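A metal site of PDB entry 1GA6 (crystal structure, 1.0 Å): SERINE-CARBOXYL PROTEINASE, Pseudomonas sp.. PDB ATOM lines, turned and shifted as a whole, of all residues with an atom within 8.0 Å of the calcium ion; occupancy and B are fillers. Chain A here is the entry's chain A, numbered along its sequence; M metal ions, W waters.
Within 4 Å of the calcium ion: Asp 328, Val 329, Gly 344, Gly 346 and Asp 348.
The nearest printed residue that does not touch the calcium ion is Thr 345 (4.1 Å).
Water W1 lies within hydrogen-bond range of the side-chain hydroxyl (OG1) of Thr 351, the backbone carbonyl oxygen (O) of Gly 352, the backbone NH (N) of Gly 354 and the backbone NH (N) of Val 329.
OD1 of Asp 348 lies within hydrogen-bond range of OG1 of Thr 351 (2.7 Å).
The calcium ion is bound by O of Val 329, at 2.3 Å.
OD2 of Asp 348 binds the calcium ion, 2.3 Å away.
O of Gly 346 binds the calcium ion, 2.3 Å away.
OD1 of Asp 328 binds the calcium ion (2.3 Å).
The calcium ion is bound by O of Gly 344 (2.3 Å).
Water W1 binds the calcium ion (2.4 Å).
The calcium ion has six donor atoms within binding distance.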
ATOM      1  N   VAL A 219      22.464 -20.085  21.008  1.00  0.00           N
ATOM      2  CA  VAL A 219      21.443 -21.107  21.280  1.00  0.00           C
ATOM      3  C   VAL A 219      21.785 -21.873  22.521  1.00  0.00           C
ATOM      4  O   VAL A 219      22.949 -22.207  22.762  1.00  0.00           O
ATOM      5  CB  VAL A 219      21.349 -22.047  20.061  1.00  0.00           C
ATOM      6  CG1 VAL A 219      20.386 -23.199  20.314  1.00  0.00           C
ATOM      7  CG2 VAL A 219      20.948 -21.297  18.811  1.00  0.00           C
ATOM      8  N   VAL A 326      14.997  -6.555  19.838  1.00  0.00           N
ATOM      9  CA  VAL A 326      15.462  -7.858  20.285  1.00  0.00           C
ATOM     10  C   VAL A 326      16.968  -7.957  20.202  1.00  0.00           C
ATOM     11  O   VAL A 326      17.645  -7.262  19.451  1.00  0.00           O
ATOM     12  CB  VAL A 326      14.811  -9.018  19.494  1.00  0.00           C
ATOM     13  CG1 VAL A 326      13.326  -9.066  19.753  1.00  0.00           C
ATOM     14  CG2 VAL A 326      15.118  -8.920  17.998  1.00  0.00           C
ATOM     15  N   HIS A 327      17.481  -8.939  20.960  1.00  0.00           N
ATOM     16  CA  HIS A 327      18.793  -9.518  20.762  1.00  0.00           C
ATOM     17  C   HIS A 327      18.627 -10.723  19.864  1.00  0.00           C
ATOM     18  O   HIS A 327      18.085 -11.753  20.271  1.00  0.00           O
ATOM     19  CB  HIS A 327      19.414  -9.933  22.084  1.00  0.00           C
ATOM     20  CG  HIS A 327      19.591  -8.856  23.053  1.00  0.00           C
ATOM     21  ND1 HIS A 327      20.524  -7.838  22.897  1.00  0.00           N
ATOM     22  CD2 HIS A 327      19.043  -8.596  24.250  1.00  0.00           C
ATOM     23  CE1 HIS A 327      20.537  -7.027  23.921  1.00  0.00           C
ATOM     24  NE2 HIS A 327      19.620  -7.452  24.772  1.00  0.00           N
ATOM     25  N   ASP A 328      19.063 -10.596  18.616  1.00  0.00           N
ATOM     26  CA  ASP A 328      18.909 -11.620  17.611  1.00  0.00           C
ATOM     27  C   ASP A 328      19.970 -12.685  17.781  1.00  0.00           C
ATOM     28  O   ASP A 328      21.148 -12.463  17.483  1.00  0.00           O
ATOM     29  CB  ASP A 328      19.035 -10.986  16.212  1.00  0.00           C
ATOM     30  CG  ASP A 328      18.827 -11.979  15.077  1.00  0.00           C
ATOM     31  OD1 ASP A 328      18.253 -13.055  15.349  1.00  0.00           O
ATOM     32  OD2 ASP A 328      19.237 -11.636  13.926  1.00  0.00           O
ATOM     33  N   VAL A 329      19.577 -13.883  18.221  1.00  0.00           N
ATOM     34  CA  VAL A 329      20.534 -14.975  18.362  1.00  0.00           C
ATOM     35  C   VAL A 329      20.907 -15.474  16.984  1.00  0.00           C
ATOM     36  O   VAL A 329      20.003 -15.710  16.139  1.00  0.00           O
ATOM     37  CB  VAL A 329      19.938 -16.087  19.235  1.00  0.00           C
ATOM     38  CG1 VAL A 329      20.890 -17.261  19.313  1.00  0.00           C
ATOM     39  CG2 VAL A 329      19.585 -15.540  20.627  1.00  0.00           C
ATOM     40  N   LYS A 330      22.192 -15.665  16.713  1.00  0.00           N
ATOM     41  CA  LYS A 330      22.704 -16.044  15.422  1.00  0.00           C
ATOM     42  C   LYS A 330      23.501 -17.325  15.373  1.00  0.00           C
ATOM     43  O   LYS A 330      23.690 -17.892  14.310  1.00  0.00           O
ATOM     44  CB  LYS A 330      23.500 -14.915  14.764  1.00  0.00           C
ATOM     45  CG  LYS A 330      22.617 -13.659  14.481  1.00  0.00           C
ATOM     46  CD  LYS A 330      23.426 -12.589  13.781  1.00  0.00           C
ATOM     47  CE  LYS A 330      22.649 -11.380  13.429  1.00  0.00           C
ATOM     48  NZ  LYS A 330      23.499 -10.405  12.648  1.00  0.00           N
ATOM     49  N   SER A 331      24.044 -17.789  16.533  1.00  0.00           N
ATOM     50  CA  SER A 331      24.964 -18.903  16.560  1.00  0.00           C
ATOM     51  C   SER A 331      24.390 -20.079  17.371  1.00  0.00           C
ATOM     52  O   SER A 331      23.935 -19.870  18.510  1.00  0.00           O
ATOM     53  CB  SER A 331      26.253 -18.465  17.253  1.00  0.00           C
ATOM     54  OG  SER A 331      27.172 -19.521  17.472  1.00  0.00           O
ATOM     55  N   ASN A 342      19.462 -24.615  12.875  1.00  0.00           N
ATOM     56  CA  ASN A 342      20.523 -23.647  13.168  1.00  0.00           C
ATOM     57  C   ASN A 342      19.915 -22.272  13.396  1.00  0.00           C
ATOM     58  O   ASN A 342      18.989 -21.852  12.703  1.00  0.00           O
ATOM     59  CB  ASN A 342      21.499 -23.570  11.982  1.00  0.00           C
ATOM     60  CG  ASN A 342      22.156 -24.916  11.776  1.00  0.00           C
ATOM     61  OD1 ASN A 342      22.805 -25.451  12.625  1.00  0.00           O
ATOM     62  ND2 ASN A 342      21.890 -25.494  10.597  1.00  0.00           N
ATOM     63  N   ALA A 343      20.517 -21.519  14.320  1.00  0.00           N
ATOM     64  CA  ALA A 343      20.161 -20.113  14.441  1.00  0.00           C
ATOM     65  C   ALA A 343      20.664 -19.356  13.228  1.00  0.00           C
ATOM     66  O   ALA A 343      21.552 -19.819  12.466  1.00  0.00           O
ATOM     67  CB  ALA A 343      20.729 -19.524  15.722  1.00  0.00           C
ATOM     68  N   GLY A 344      20.094 -18.178  13.019  1.00  0.00           N
ATOM     69  CA  GLY A 344      20.507 -17.358  11.916  1.00  0.00           C
ATOM     70  C   GLY A 344      19.937 -15.959  12.053  1.00  0.00           C
ATOM     71  O   GLY A 344      19.362 -15.600  13.085  1.00  0.00           O
ATOM     72  N   THR A 345      20.112 -15.152  11.018  1.00  0.00           N
ATOM     73  CA  THR A 345      19.619 -13.790  11.057  1.00  0.00           C
ATOM     74  C   THR A 345      18.105 -13.792  11.156  1.00  0.00           C
ATOM     75  O   THR A 345      17.409 -14.495  10.414  1.00  0.00           O
ATOM     76  CB  THR A 345      20.042 -13.088   9.733  1.00  0.00           C
ATOM     77  OG1 THR A 345      21.492 -13.089   9.748  1.00  0.00           O
ATOM     78  CG2 THR A 345      19.491 -11.665   9.655  1.00  0.00           C
ATOM     79  N   GLY A 346      17.581 -12.963  12.074  1.00  0.00           N
ATOM     80  CA  GLY A 346      16.149 -12.897  12.257  1.00  0.00           C
ATOM     81  C   GLY A 346      15.542 -14.118  12.932  1.00  0.00           C
ATOM     82  O   GLY A 346      16.205 -14.810  13.728  1.00  0.00           O
ATOM     83  N   TRP A 347      14.269 -14.369  12.662  1.00  0.00           N
ATOM     84  CA  TRP A 347      13.580 -15.463  13.328  1.00  0.00           C
ATOM     85  C   TRP A 347      14.224 -16.781  12.928  1.00  0.00           C
ATOM     86  O   TRP A 347      14.488 -17.008  11.737  1.00  0.00           O
ATOM     87  CB  TRP A 347      12.078 -15.434  12.904  1.00  0.00           C
ATOM     88  CG  TRP A 347      11.228 -16.343  13.747  1.00  0.00           C
ATOM     89  CD1 TRP A 347      10.435 -15.968  14.816  1.00  0.00           C
ATOM     90  CD2 TRP A 347      11.066 -17.776  13.639  1.00  0.00           C
ATOM     91  NE1 TRP A 347       9.836 -17.058  15.353  1.00  0.00           N
ATOM     92  CE2 TRP A 347      10.203 -18.184  14.667  1.00  0.00           C
ATOM     93  CE3 TRP A 347      11.590 -18.747  12.767  1.00  0.00           C
ATOM     94  CZ2 TRP A 347       9.883 -19.522  14.858  1.00  0.00           C
ATOM     95  CZ3 TRP A 347      11.251 -20.069  12.962  1.00  0.00           C
ATOM     96  CH2 TRP A 347      10.406 -20.430  14.017  1.00  0.00           C
ATOM     97  N   ASP A 348      14.439 -17.669  13.889  1.00  0.00           N
ATOM     98  CA  ASP A 348      14.965 -19.012  13.589  1.00  0.00           C
ATOM     99  C   ASP A 348      14.284 -20.019  14.488  1.00  0.00           C
ATOM    100  O   ASP A 348      13.601 -19.696  15.482  1.00  0.00           O
ATOM    101  CB  ASP A 348      16.486 -19.041  13.666  1.00  0.00           C
ATOM    102  CG  ASP A 348      17.037 -18.592  15.011  1.00  0.00           C
ATOM    103  OD1 ASP A 348      16.668 -19.171  16.047  1.00  0.00           O
ATOM    104  OD2 ASP A 348      17.869 -17.635  14.986  1.00  0.00           O
ATOM    105  N   TYR A 349      14.409 -21.311  14.111  1.00  0.00           N
ATOM    106  CA  TYR A 349      13.711 -22.328  14.851  1.00  0.00           C
ATOM    107  C   TYR A 349      14.253 -22.578  16.254  1.00  0.00           C
ATOM    108  O   TYR A 349      13.455 -22.909  17.141  1.00  0.00           O
ATOM    109  CB  TYR A 349      13.685 -23.639  14.045  1.00  0.00           C
ATOM    110  CG  TYR A 349      12.745 -23.614  12.871  1.00  0.00           C
ATOM    111  CD1 TYR A 349      11.356 -23.650  13.091  1.00  0.00           C
ATOM    112  CD2 TYR A 349      13.185 -23.535  11.564  1.00  0.00           C
ATOM    113  CE1 TYR A 349      10.442 -23.636  12.040  1.00  0.00           C
ATOM    114  CE2 TYR A 349      12.288 -23.507  10.511  1.00  0.00           C
ATOM    115  CZ  TYR A 349      10.932 -23.552  10.746  1.00  0.00           C
ATOM    116  OH  TYR A 349       9.992 -23.547   9.718  1.00  0.00           O
ATOM    117  N   PRO A 350      15.560 -22.426  16.552  1.00  0.00           N
ATOM    118  CA  PRO A 350      15.957 -22.666  17.938  1.00  0.00           C
ATOM    119  C   PRO A 350      15.430 -21.598  18.916  1.00  0.00           C
ATOM    120  O   PRO A 350      15.168 -21.906  20.086  1.00  0.00           O
ATOM    121  CB  PRO A 350      17.471 -22.692  17.882  1.00  0.00           C
ATOM    122  CG  PRO A 350      17.763 -23.218  16.474  1.00  0.00           C
ATOM    123  CD  PRO A 350      16.728 -22.462  15.640  1.00  0.00           C
ATOM    124  N   THR A 351      15.379 -20.340  18.454  1.00  0.00           N
ATOM    125  CA  THR A 351      15.209 -19.221  19.361  1.00  0.00           C
ATOM    126  C   THR A 351      14.119 -18.242  18.989  1.00  0.00           C
ATOM    127  O   THR A 351      13.887 -17.265  19.728  1.00  0.00           O
ATOM    128  CB  THR A 351      16.533 -18.449  19.607  1.00  0.00           C
ATOM    129  OG1 THR A 351      17.011 -17.847  18.389  1.00  0.00           O
ATOM    130  CG2 THR A 351      17.575 -19.339  20.217  1.00  0.00           C
ATOM    131  N   GLY A 352      13.417 -18.431  17.878  1.00  0.00           N
ATOM    132  CA  GLY A 352      12.418 -17.474  17.450  1.00  0.00           C
ATOM    133  C   GLY A 352      13.066 -16.142  17.178  1.00  0.00           C
ATOM    134  O   GLY A 352      14.113 -16.063  16.524  1.00  0.00           O
ATOM    135  N   TRP A 353      12.483 -15.044  17.680  1.00  0.00           N
ATOM    136  CA  TRP A 353      13.040 -13.727  17.471  1.00  0.00           C
ATOM    137  C   TRP A 353      14.250 -13.429  18.371  1.00  0.00           C
ATOM    138  O   TRP A 353      14.857 -12.365  18.195  1.00  0.00           O
ATOM    139  CB  TRP A 353      11.969 -12.655  17.724  1.00  0.00           C
ATOM    140  CG  TRP A 353      10.889 -12.636  16.696  1.00  0.00           C
ATOM    141  CD1 TRP A 353       9.571 -12.943  16.901  1.00  0.00           C
ATOM    142  CD2 TRP A 353      11.007 -12.270  15.320  1.00  0.00           C
ATOM    143  NE1 TRP A 353       8.863 -12.787  15.743  1.00  0.00           N
ATOM    144  CE2 TRP A 353       9.727 -12.376  14.746  1.00  0.00           C
ATOM    145  CE3 TRP A 353      12.092 -11.845  14.507  1.00  0.00           C
ATOM    146  CZ2 TRP A 353       9.490 -12.087  13.390  1.00  0.00           C
ATOM    147  CZ3 TRP A 353      11.854 -11.576  13.186  1.00  0.00           C
ATOM    148  CH2 TRP A 353      10.571 -11.690  12.633  1.00  0.00           C
ATOM    149  N   GLY A 354      14.549 -14.283  19.341  1.00  0.00           N
ATOM    150  CA  GLY A 354      15.580 -14.003  20.339  1.00  0.00           C
ATOM    151  C   GLY A 354      14.964 -13.364  21.584  1.00  0.00           C
ATOM    152  O   GLY A 354      13.763 -13.536  21.848  1.00  0.00           O
HETATM  153 CA    CA M   1      18.053 -15.341  14.994  1.00  0.00          CA
HETATM  154  O   HOH W   1      16.778 -15.424  17.044  1.00  0.00           O
